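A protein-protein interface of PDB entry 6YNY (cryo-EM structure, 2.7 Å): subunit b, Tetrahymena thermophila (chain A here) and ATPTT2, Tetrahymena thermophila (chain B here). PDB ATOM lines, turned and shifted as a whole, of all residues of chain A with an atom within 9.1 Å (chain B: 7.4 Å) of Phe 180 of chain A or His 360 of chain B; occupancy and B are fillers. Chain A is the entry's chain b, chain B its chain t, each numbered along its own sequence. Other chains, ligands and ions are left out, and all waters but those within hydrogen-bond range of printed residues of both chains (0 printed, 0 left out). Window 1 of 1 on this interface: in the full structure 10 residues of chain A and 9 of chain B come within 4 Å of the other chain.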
ATOM      1  N   ARG A 172     -16.617 -22.738  34.635  1.00  0.00           N
ATOM      2  CA  ARG A 172     -17.694 -22.793  33.657  1.00  0.00           C
ATOM      3  C   ARG A 172     -17.473 -21.795  32.531  1.00  0.00           C
ATOM      4  O   ARG A 172     -17.878 -22.049  31.393  1.00  0.00           O
ATOM      5  CB  ARG A 172     -19.036 -22.541  34.347  1.00  0.00           C
ATOM      6  CG  ARG A 172     -19.092 -23.106  35.748  1.00  0.00           C
ATOM      7  CD  ARG A 172     -20.493 -23.312  36.297  1.00  0.00           C
ATOM      8  NE  ARG A 172     -21.154 -22.081  36.716  1.00  0.00           N
ATOM      9  CZ  ARG A 172     -22.116 -22.031  37.633  1.00  0.00           C
ATOM     10  NH1 ARG A 172     -22.513 -23.140  38.238  1.00  0.00           N
ATOM     11  NH2 ARG A 172     -22.678 -20.873  37.954  1.00  0.00           N
ATOM     12  N   ARG A 173     -16.817 -20.672  32.825  1.00  0.00           N
ATOM     13  CA  ARG A 173     -16.483 -19.710  31.784  1.00  0.00           C
ATOM     14  C   ARG A 173     -15.361 -20.230  30.895  1.00  0.00           C
ATOM     15  O   ARG A 173     -15.433 -20.119  29.667  1.00  0.00           O
ATOM     16  CB  ARG A 173     -16.075 -18.381  32.411  1.00  0.00           C
ATOM     17  CG  ARG A 173     -17.051 -17.822  33.419  1.00  0.00           C
ATOM     18  CD  ARG A 173     -18.364 -17.481  32.786  1.00  0.00           C
ATOM     19  NE  ARG A 173     -19.264 -16.819  33.723  1.00  0.00           N
ATOM     20  CZ  ARG A 173     -20.057 -17.456  34.578  1.00  0.00           C
ATOM     21  NH1 ARG A 173     -20.070 -18.780  34.639  1.00  0.00           N
ATOM     22  NH2 ARG A 173     -20.843 -16.760  35.378  1.00  0.00           N
ATOM     23  N   ALA A 174     -14.319 -20.802  31.501  1.00  0.00           N
ATOM     24  CA  ALA A 174     -13.181 -21.280  30.724  1.00  0.00           C
ATOM     25  C   ALA A 174     -13.594 -22.382  29.761  1.00  0.00           C
ATOM     26  O   ALA A 174     -13.109 -22.441  28.626  1.00  0.00           O
ATOM     27  CB  ALA A 174     -12.084 -21.773  31.663  1.00  0.00           C
ATOM     28  N   ALA A 175     -14.485 -23.269  30.197  1.00  0.00           N
ATOM     29  CA  ALA A 175     -14.965 -24.324  29.315  1.00  0.00           C
ATOM     30  C   ALA A 175     -15.818 -23.756  28.191  1.00  0.00           C
ATOM     31  O   ALA A 175     -15.772 -24.247  27.058  1.00  0.00           O
ATOM     32  CB  ALA A 175     -15.749 -25.357  30.116  1.00  0.00           C
ATOM     33  N   ALA A 176     -16.609 -22.726  28.487  1.00  0.00           N
ATOM     34  CA  ALA A 176     -17.405 -22.084  27.450  1.00  0.00           C
ATOM     35  C   ALA A 176     -16.524 -21.350  26.449  1.00  0.00           C
ATOM     36  O   ALA A 176     -16.809 -21.351  25.247  1.00  0.00           O
ATOM     37  CB  ALA A 176     -18.400 -21.118  28.088  1.00  0.00           C
ATOM     38  N   ASN A 177     -15.454 -20.716  26.926  1.00  0.00           N
ATOM     39  CA  ASN A 177     -14.569 -19.981  26.034  1.00  0.00           C
ATOM     40  C   ASN A 177     -13.829 -20.911  25.085  1.00  0.00           C
ATOM     41  O   ASN A 177     -13.570 -20.543  23.936  1.00  0.00           O
ATOM     42  CB  ASN A 177     -13.580 -19.158  26.854  1.00  0.00           C
ATOM     43  CG  ASN A 177     -12.843 -18.136  26.023  1.00  0.00           C
ATOM     44  OD1 ASN A 177     -13.384 -17.082  25.697  1.00  0.00           O
ATOM     45  ND2 ASN A 177     -11.599 -18.432  25.688  1.00  0.00           N
ATOM     46  N   GLU A 178     -13.481 -22.111  25.546  1.00  0.00           N
ATOM     47  CA  GLU A 178     -12.829 -23.074  24.669  1.00  0.00           C
ATOM     48  C   GLU A 178     -13.809 -23.639  23.653  1.00  0.00           C
ATOM     49  O   GLU A 178     -13.455 -23.848  22.489  1.00  0.00           O
ATOM     50  CB  GLU A 178     -12.203 -24.191  25.498  1.00  0.00           C
ATOM     51  CG  GLU A 178     -11.479 -25.239  24.685  1.00  0.00           C
ATOM     52  CD  GLU A 178     -10.605 -26.136  25.536  1.00  0.00           C
ATOM     53  OE1 GLU A 178     -10.871 -26.252  26.751  1.00  0.00           O
ATOM     54  OE2 GLU A 178      -9.646 -26.720  24.994  1.00  0.00           O
ATOM     55  N   ILE A 179     -15.051 -23.882  24.072  1.00  0.00           N
ATOM     56  CA  ILE A 179     -16.070 -24.355  23.144  1.00  0.00           C
ATOM     57  C   ILE A 179     -16.412 -23.276  22.128  1.00  0.00           C
ATOM     58  O   ILE A 179     -16.586 -23.559  20.939  1.00  0.00           O
ATOM     59  CB  ILE A 179     -17.315 -24.812  23.921  1.00  0.00           C
ATOM     60  CG1 ILE A 179     -16.984 -26.041  24.762  1.00  0.00           C
ATOM     61  CG2 ILE A 179     -18.452 -25.094  22.972  1.00  0.00           C
ATOM     62  CD1 ILE A 179     -18.043 -26.417  25.730  1.00  0.00           C
ATOM     63  N   PHE A 180     -16.521 -22.027  22.578  1.00  0.00           N
ATOM     64  CA  PHE A 180     -16.760 -20.929  21.650  1.00  0.00           C
ATOM     65  C   PHE A 180     -15.673 -20.867  20.590  1.00  0.00           C
ATOM     66  O   PHE A 180     -15.948 -20.574  19.421  1.00  0.00           O
ATOM     67  CB  PHE A 180     -16.834 -19.610  22.414  1.00  0.00           C
ATOM     68  CG  PHE A 180     -16.851 -18.397  21.535  1.00  0.00           C
ATOM     69  CD1 PHE A 180     -18.042 -17.873  21.080  1.00  0.00           C
ATOM     70  CD2 PHE A 180     -15.674 -17.775  21.168  1.00  0.00           C
ATOM     71  CE1 PHE A 180     -18.057 -16.762  20.276  1.00  0.00           C
ATOM     72  CE2 PHE A 180     -15.691 -16.666  20.363  1.00  0.00           C
ATOM     73  CZ  PHE A 180     -16.881 -16.160  19.919  1.00  0.00           C
ATOM     74  N   THR A 181     -14.431 -21.150  20.980  1.00  0.00           N
ATOM     75  CA  THR A 181     -13.330 -21.112  20.030  1.00  0.00           C
ATOM     76  C   THR A 181     -13.386 -22.294  19.071  1.00  0.00           C
ATOM     77  O   THR A 181     -13.066 -22.152  17.887  1.00  0.00           O
ATOM     78  CB  THR A 181     -12.005 -21.087  20.788  1.00  0.00           C
ATOM     79  OG1 THR A 181     -12.043 -20.064  21.789  1.00  0.00           O
ATOM     80  CG2 THR A 181     -10.865 -20.807  19.857  1.00  0.00           C
ATOM     81  N   MET A 182     -13.802 -23.464  19.556  1.00  0.00           N
ATOM     82  CA  MET A 182     -13.950 -24.613  18.669  1.00  0.00           C
ATOM     83  C   MET A 182     -15.047 -24.378  17.640  1.00  0.00           C
ATOM     84  O   MET A 182     -14.889 -24.735  16.468  1.00  0.00           O
ATOM     85  CB  MET A 182     -14.244 -25.869  19.480  1.00  0.00           C
ATOM     86  CG  MET A 182     -13.102 -26.313  20.359  1.00  0.00           C
ATOM     87  SD  MET A 182     -13.460 -27.815  21.280  1.00  0.00           S
ATOM     88  CE  MET A 182     -13.588 -28.979  19.929  1.00  0.00           C
ATOM     89  N   GLU A 183     -16.168 -23.790  18.057  1.00  0.00           N
ATOM     90  CA  GLU A 183     -17.216 -23.448  17.105  1.00  0.00           C
ATOM     91  C   GLU A 183     -16.706 -22.476  16.053  1.00  0.00           C
ATOM     92  O   GLU A 183     -17.125 -22.536  14.892  1.00  0.00           O
ATOM     93  CB  GLU A 183     -18.416 -22.853  17.838  1.00  0.00           C
ATOM     94  CG  GLU A 183     -19.055 -23.776  18.860  1.00  0.00           C
ATOM     95  CD  GLU A 183     -19.819 -24.925  18.234  1.00  0.00           C
ATOM     96  OE1 GLU A 183     -19.641 -25.179  17.026  1.00  0.00           O
ATOM     97  OE2 GLU A 183     -20.605 -25.576  18.954  1.00  0.00           O
ATOM     98  N   ALA A 184     -15.802 -21.575  16.439  1.00  0.00           N
ATOM     99  CA  ALA A 184     -15.227 -20.639  15.485  1.00  0.00           C
ATOM    100  C   ALA A 184     -14.386 -21.348  14.434  1.00  0.00           C
ATOM    101  O   ALA A 184     -14.259 -20.855  13.309  1.00  0.00           O
ATOM    102  CB  ALA A 184     -14.388 -19.600  16.221  1.00  0.00           C
ATOM    103  N   PHE A 185     -13.798 -22.492  14.780  1.00  0.00           N
ATOM    104  CA  PHE A 185     -12.995 -23.279  13.855  1.00  0.00           C
ATOM    105  C   PHE A 185     -13.696 -24.570  13.444  1.00  0.00           C
ATOM    106  O   PHE A 185     -13.039 -25.573  13.160  1.00  0.00           O
ATOM    107  CB  PHE A 185     -11.632 -23.595  14.463  1.00  0.00           C
ATOM    108  CG  PHE A 185     -10.773 -22.391  14.687  1.00  0.00           C
ATOM    109  CD1 PHE A 185      -9.996 -21.884  13.668  1.00  0.00           C
ATOM    110  CD2 PHE A 185     -10.732 -21.773  15.919  1.00  0.00           C
ATOM    111  CE1 PHE A 185      -9.205 -20.781  13.874  1.00  0.00           C
ATOM    112  CE2 PHE A 185      -9.944 -20.675  16.126  1.00  0.00           C
ATOM    113  CZ  PHE A 185      -9.181 -20.177  15.103  1.00  0.00           C
ATOM    114  N   TYR A 186     -15.029 -24.563  13.411  1.00  0.00           N
ATOM    115  CA  TYR A 186     -15.755 -25.756  12.991  1.00  0.00           C
ATOM    116  C   TYR A 186     -15.456 -26.101  11.540  1.00  0.00           C
ATOM    117  O   TYR A 186     -15.283 -27.276  11.196  1.00  0.00           O
ATOM    118  CB  TYR A 186     -17.256 -25.560  13.189  1.00  0.00           C
ATOM    119  CG  TYR A 186     -18.090 -26.654  12.570  1.00  0.00           C
ATOM    120  CD1 TYR A 186     -18.244 -27.875  13.200  1.00  0.00           C
ATOM    121  CD2 TYR A 186     -18.719 -26.466  11.353  1.00  0.00           C
ATOM    122  CE1 TYR A 186     -18.999 -28.874  12.637  1.00  0.00           C
ATOM    123  CE2 TYR A 186     -19.476 -27.460  10.785  1.00  0.00           C
ATOM    124  CZ  TYR A 186     -19.612 -28.662  11.430  1.00  0.00           C
ATOM    125  OH  TYR A 186     -20.369 -29.653  10.859  1.00  0.00           O
ATOM    126  N   ALA B 328     -13.177  -5.695   8.281  1.00  0.00           N
ATOM    127  CA  ALA B 328     -11.797  -5.964   8.651  1.00  0.00           C
ATOM    128  C   ALA B 328     -11.719  -7.300   9.368  1.00  0.00           C
ATOM    129  O   ALA B 328     -12.502  -7.562  10.285  1.00  0.00           O
ATOM    130  CB  ALA B 328     -11.234  -4.855   9.544  1.00  0.00           C
ATOM    131  N   HIS B 329     -10.778  -8.136   8.945  1.00  0.00           N
ATOM    132  CA  HIS B 329     -10.524  -9.424   9.570  1.00  0.00           C
ATOM    133  C   HIS B 329      -9.045  -9.526   9.897  1.00  0.00           C
ATOM    134  O   HIS B 329      -8.197  -9.203   9.061  1.00  0.00           O
ATOM    135  CB  HIS B 329     -10.954 -10.574   8.664  1.00  0.00           C
ATOM    136  CG  HIS B 329     -12.409 -10.901   8.755  1.00  0.00           C
ATOM    137  ND1 HIS B 329     -13.389  -9.934   8.816  1.00  0.00           N
ATOM    138  CD2 HIS B 329     -13.053 -12.091   8.793  1.00  0.00           C
ATOM    139  CE1 HIS B 329     -14.573 -10.514   8.889  1.00  0.00           C
ATOM    140  NE2 HIS B 329     -14.397 -11.822   8.877  1.00  0.00           N
ATOM    141  N   PHE B 330      -8.741  -9.966  11.113  1.00  0.00           N
ATOM    142  CA  PHE B 330      -7.376 -10.071  11.602  1.00  0.00           C
ATOM    143  C   PHE B 330      -7.069 -11.518  11.957  1.00  0.00           C
ATOM    144  O   PHE B 330      -7.857 -12.175  12.644  1.00  0.00           O
ATOM    145  CB  PHE B 330      -7.158  -9.173  12.815  1.00  0.00           C
ATOM    146  CG  PHE B 330      -7.347  -7.719  12.532  1.00  0.00           C
ATOM    147  CD1 PHE B 330      -8.597  -7.141  12.603  1.00  0.00           C
ATOM    148  CD2 PHE B 330      -6.269  -6.926  12.203  1.00  0.00           C
ATOM    149  CE1 PHE B 330      -8.766  -5.807  12.345  1.00  0.00           C
ATOM    150  CE2 PHE B 330      -6.437  -5.590  11.945  1.00  0.00           C
ATOM    151  CZ  PHE B 330      -7.687  -5.030  12.017  1.00  0.00           C
ATOM    152  N   VAL B 355     -15.435  -4.057  13.683  1.00  0.00           N
ATOM    153  CA  VAL B 355     -14.863  -5.281  14.232  1.00  0.00           C
ATOM    154  C   VAL B 355     -15.708  -5.740  15.410  1.00  0.00           C
ATOM    155  O   VAL B 355     -15.866  -5.019  16.402  1.00  0.00           O
ATOM    156  CB  VAL B 355     -13.402  -5.065  14.637  1.00  0.00           C
ATOM    157  CG1 VAL B 355     -12.929  -6.174  15.544  1.00  0.00           C
ATOM    158  CG2 VAL B 355     -12.541  -5.007  13.408  1.00  0.00           C
ATOM    159  N   LYS B 356     -16.255  -6.950  15.300  1.00  0.00           N
ATOM    160  CA  LYS B 356     -17.111  -7.492  16.347  1.00  0.00           C
ATOM    161  C   LYS B 356     -16.291  -7.994  17.527  1.00  0.00           C
ATOM    162  O   LYS B 356     -16.605  -7.694  18.683  1.00  0.00           O
ATOM    163  CB  LYS B 356     -17.974  -8.615  15.777  1.00  0.00           C
ATOM    164  CG  LYS B 356     -18.997  -9.157  16.742  1.00  0.00           C
ATOM    165  CD  LYS B 356     -20.079  -9.930  16.016  1.00  0.00           C
ATOM    166  CE  LYS B 356     -20.916 -10.743  16.976  1.00  0.00           C
ATOM    167  NZ  LYS B 356     -21.319  -9.953  18.157  1.00  0.00           N
ATOM    168  N   GLY B 357     -15.244  -8.752  17.257  1.00  0.00           N
ATOM    169  CA  GLY B 357     -14.353  -9.202  18.299  1.00  0.00           C
ATOM    170  C   GLY B 357     -13.789 -10.572  17.989  1.00  0.00           C
ATOM    171  O   GLY B 357     -13.937 -11.096  16.889  1.00  0.00           O
ATOM    172  N   PHE B 358     -13.134 -11.134  18.998  1.00  0.00           N
ATOM    173  CA  PHE B 358     -12.501 -12.437  18.865  1.00  0.00           C
ATOM    174  C   PHE B 358     -13.522 -13.495  18.476  1.00  0.00           C
ATOM    175  O   PHE B 358     -14.633 -13.542  19.011  1.00  0.00           O
ATOM    176  CB  PHE B 358     -11.822 -12.809  20.176  1.00  0.00           C
ATOM    177  CG  PHE B 358     -11.171 -14.151  20.167  1.00  0.00           C
ATOM    178  CD1 PHE B 358      -9.899 -14.306  19.657  1.00  0.00           C
ATOM    179  CD2 PHE B 358     -11.822 -15.254  20.676  1.00  0.00           C
ATOM    180  CE1 PHE B 358      -9.293 -15.533  19.650  1.00  0.00           C
ATOM    181  CE2 PHE B 358     -11.219 -16.490  20.670  1.00  0.00           C
ATOM    182  CZ  PHE B 358      -9.950 -16.628  20.156  1.00  0.00           C
ATOM    183  N   GLY B 359     -13.136 -14.349  17.533  1.00  0.00           N
ATOM    184  CA  GLY B 359     -13.976 -15.429  17.076  1.00  0.00           C
ATOM    185  C   GLY B 359     -14.888 -15.086  15.921  1.00  0.00           C
ATOM    186  O   GLY B 359     -15.442 -16.001  15.301  1.00  0.00           O
ATOM    187  N   HIS B 360     -15.069 -13.804  15.615  1.00  0.00           N
ATOM    188  CA  HIS B 360     -15.879 -13.368  14.487  1.00  0.00           C
ATOM    189  C   HIS B 360     -15.052 -12.665  13.424  1.00  0.00           C
ATOM    190  O   HIS B 360     -15.121 -13.022  12.245  1.00  0.00           O
ATOM    191  CB  HIS B 360     -16.993 -12.433  14.971  1.00  0.00           C
ATOM    192  CG  HIS B 360     -17.798 -12.986  16.103  1.00  0.00           C
ATOM    193  ND1 HIS B 360     -17.523 -12.697  17.420  1.00  0.00           N
ATOM    194  CD2 HIS B 360     -18.869 -13.812  16.113  1.00  0.00           C
ATOM    195  CE1 HIS B 360     -18.394 -13.318  18.194  1.00  0.00           C
ATOM    196  NE2 HIS B 360     -19.221 -14.002  17.426  1.00  0.00           N
ATOM    197  N   ASP B 361     -14.264 -11.670  13.819  1.00  0.00           N
ATOM    198  CA  ASP B 361     -13.383 -10.958  12.914  1.00  0.00           C
ATOM    199  C   ASP B 361     -11.921 -11.053  13.314  1.00  0.00           C
ATOM    200  O   ASP B 361     -11.059 -10.605  12.550  1.00  0.00           O
ATOM    201  CB  ASP B 361     -13.781  -9.476  12.836  1.00  0.00           C
ATOM    202  CG  ASP B 361     -15.237  -9.278  12.477  1.00  0.00           C
ATOM    203  OD1 ASP B 361     -16.093  -9.401  13.378  1.00  0.00           O
ATOM    204  OD2 ASP B 361     -15.530  -8.997  11.297  1.00  0.00           O
ATOM    205  N   ILE B 362     -11.619 -11.617  14.479  1.00  0.00           N
ATOM    206  CA  ILE B 362     -10.261 -11.740  14.990  1.00  0.00           C
ATOM    207  C   ILE B 362     -10.046 -13.192  15.382  1.00  0.00           C
ATOM    208  O   ILE B 362     -10.804 -13.736  16.192  1.00  0.00           O
ATOM    209  CB  ILE B 362     -10.010 -10.817  16.192  1.00  0.00           C
ATOM    210  CG1 ILE B 362     -10.280  -9.363  15.818  1.00  0.00           C
ATOM    211  CG2 ILE B 362      -8.593 -10.971  16.684  1.00  0.00           C
ATOM    212  CD1 ILE B 362     -10.465  -8.470  16.994  1.00  0.00           C
ATOM    213  N   PHE B 363      -9.019 -13.814  14.815  1.00  0.00           N
ATOM    214  CA  PHE B 363      -8.702 -15.204  15.090  1.00  0.00           C
ATOM    215  C   PHE B 363      -7.215 -15.339  15.364  1.00  0.00           C
ATOM    216  O   PHE B 363      -6.409 -14.527  14.908  1.00  0.00           O
ATOM    217  CB  PHE B 363      -9.070 -16.115  13.916  1.00  0.00           C
ATOM    218  CG  PHE B 363     -10.451 -15.904  13.390  1.00  0.00           C
ATOM    219  CD1 PHE B 363     -11.493 -16.710  13.798  1.00  0.00           C
ATOM    220  CD2 PHE B 363     -10.706 -14.903  12.476  1.00  0.00           C
ATOM    221  CE1 PHE B 363     -12.762 -16.516  13.309  1.00  0.00           C
ATOM    222  CE2 PHE B 363     -11.967 -14.705  11.989  1.00  0.00           C
ATOM    223  CZ  PHE B 363     -12.999 -15.511  12.403  1.00  0.00           C
ATOM    224  N   LYS B 389      -9.644 -18.924   6.314  1.00  0.00           N
ATOM    225  CA  LYS B 389     -10.228 -17.688   6.817  1.00  0.00           C
ATOM    226  C   LYS B 389     -10.258 -16.612   5.745  1.00  0.00           C
ATOM    227  O   LYS B 389     -11.186 -15.797   5.713  1.00  0.00           O
ATOM    228  CB  LYS B 389      -9.454 -17.197   8.034  1.00  0.00           C
ATOM    229  CG  LYS B 389      -9.479 -18.151   9.205  1.00  0.00           C
ATOM    230  CD  LYS B 389     -10.888 -18.396   9.689  1.00  0.00           C
ATOM    231  CE  LYS B 389     -10.902 -19.213  10.949  1.00  0.00           C
ATOM    232  NZ  LYS B 389     -12.281 -19.536  11.357  1.00  0.00           N
ATOM    233  N   TYR B 397     -17.983 -12.121   3.637  1.00  0.00           N
ATOM    234  CA  TYR B 397     -17.917 -10.909   4.444  1.00  0.00           C
ATOM    235  C   TYR B 397     -17.368  -9.693   3.719  1.00  0.00           C
ATOM    236  O   TYR B 397     -17.787  -8.577   4.023  1.00  0.00           O
ATOM    237  CB  TYR B 397     -17.068 -11.147   5.695  1.00  0.00           C
ATOM    238  CG  TYR B 397     -17.580 -12.258   6.565  1.00  0.00           C
ATOM    239  CD1 TYR B 397     -18.693 -12.076   7.366  1.00  0.00           C
ATOM    240  CD2 TYR B 397     -16.949 -13.487   6.592  1.00  0.00           C
ATOM    241  CE1 TYR B 397     -19.164 -13.086   8.162  1.00  0.00           C
ATOM    242  CE2 TYR B 397     -17.414 -14.504   7.384  1.00  0.00           C
ATOM    243  CZ  TYR B 397     -18.521 -14.299   8.170  1.00  0.00           C
ATOM    244  OH  TYR B 397     -18.990 -15.313   8.963  1.00  0.00           O
ATOM    245  N   LYS B 405     -25.307  -9.198   8.042  1.00  0.00           N
ATOM    246  CA  LYS B 405     -24.424 -10.206   8.616  1.00  0.00           C
ATOM    247  C   LYS B 405     -23.456 -10.739   7.571  1.00  0.00           C
ATOM    248  O   LYS B 405     -22.234 -10.646   7.728  1.00  0.00           O
ATOM    249  CB  LYS B 405     -25.247 -11.354   9.199  1.00  0.00           C
ATOM    250  CG  LYS B 405     -25.889 -11.063  10.531  1.00  0.00           C
ATOM    251  CD  LYS B 405     -24.880 -10.831  11.639  1.00  0.00           C
ATOM    252  CE  LYS B 405     -23.976 -12.013  11.838  1.00  0.00           C
ATOM    253  NZ  LYS B 405     -23.123 -11.826  13.031  1.00  0.00           N
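Phe 180 of chain A touches Phe 358 of chain B (CE2 to O, 3.6 Å).
Phe 180 of chain A touches Gly 359 of chain B (CE2 to CA, 3.9 Å).
His 360 of chain B touches Phe 180 of chain A (CE1 to CZ, 3.7 Å).
Thr 181 of chain A touches Phe 358 of chain B.
O of Gly 359 of chain B touches CB of Ala 184 of chain A, at 3.9 Å.
CE1 of Phe 185 of chain A touches CE of Lys 389 of chain B, at 3.7 Å.
The backbone carbonyl oxygen (O) of Asn 177 of chain A sits at hydrogen-bond distance from the side-chain hydroxyl (OG1) of Thr 181 of chain A, at 2.7 Å.
O of Phe 358 of chain B is in hydrogen-bond range of ND1 of His 360 of chain B (3.4 Å).
The side-chain amino group (NZ) of Lys 389 of chain B lies within hydrogen-bond range of the backbone carbonyl oxygen (O) of Ala 184 of chain A (3.1 Å).
Phe 180 of chain A touches three residues of chain B.
Of the printed residues of chain B, Phe 185 of chain A touches Lys 389 (3.7 Å).
Phe 330 of chain B touches none of the printed residues of chain A.
Gly 359 of chain B touches just these residues of chain A: Phe 180 and Ala 184.
His 360 of chain B touches one residue of chain A.
No residue of chain A comes within 4 Å of Asp 361 of chain B.
Printed residues of chain A within 4 Å of Lys 389 of chain B: Ala 184 (3.1 Å) and Phe 185 (3.7 Å).
The nearest residue of chain B that does not touch Phe 180 of chain A is Gly 357 of chain B (6.6 Å).
The nearest residue of chain A that does not touch His 360 of chain B is Ala 184 of chain A (5.9 Å).
The nearest printed residue of chain B that does not touch Ala 184 of chain A is Phe 363 of chain B (4.5 Å).
Of the 15 printed residues of chain A, 4 touch a printed residue of chain B.
Along chain B the printed residues that touch a printed residue of chain A span positions 358 to 389.
Among the printed residues, no Asp or Glu carboxylate lies within 4 Å of a Lys or Arg side-chain nitrogen of the other chain.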
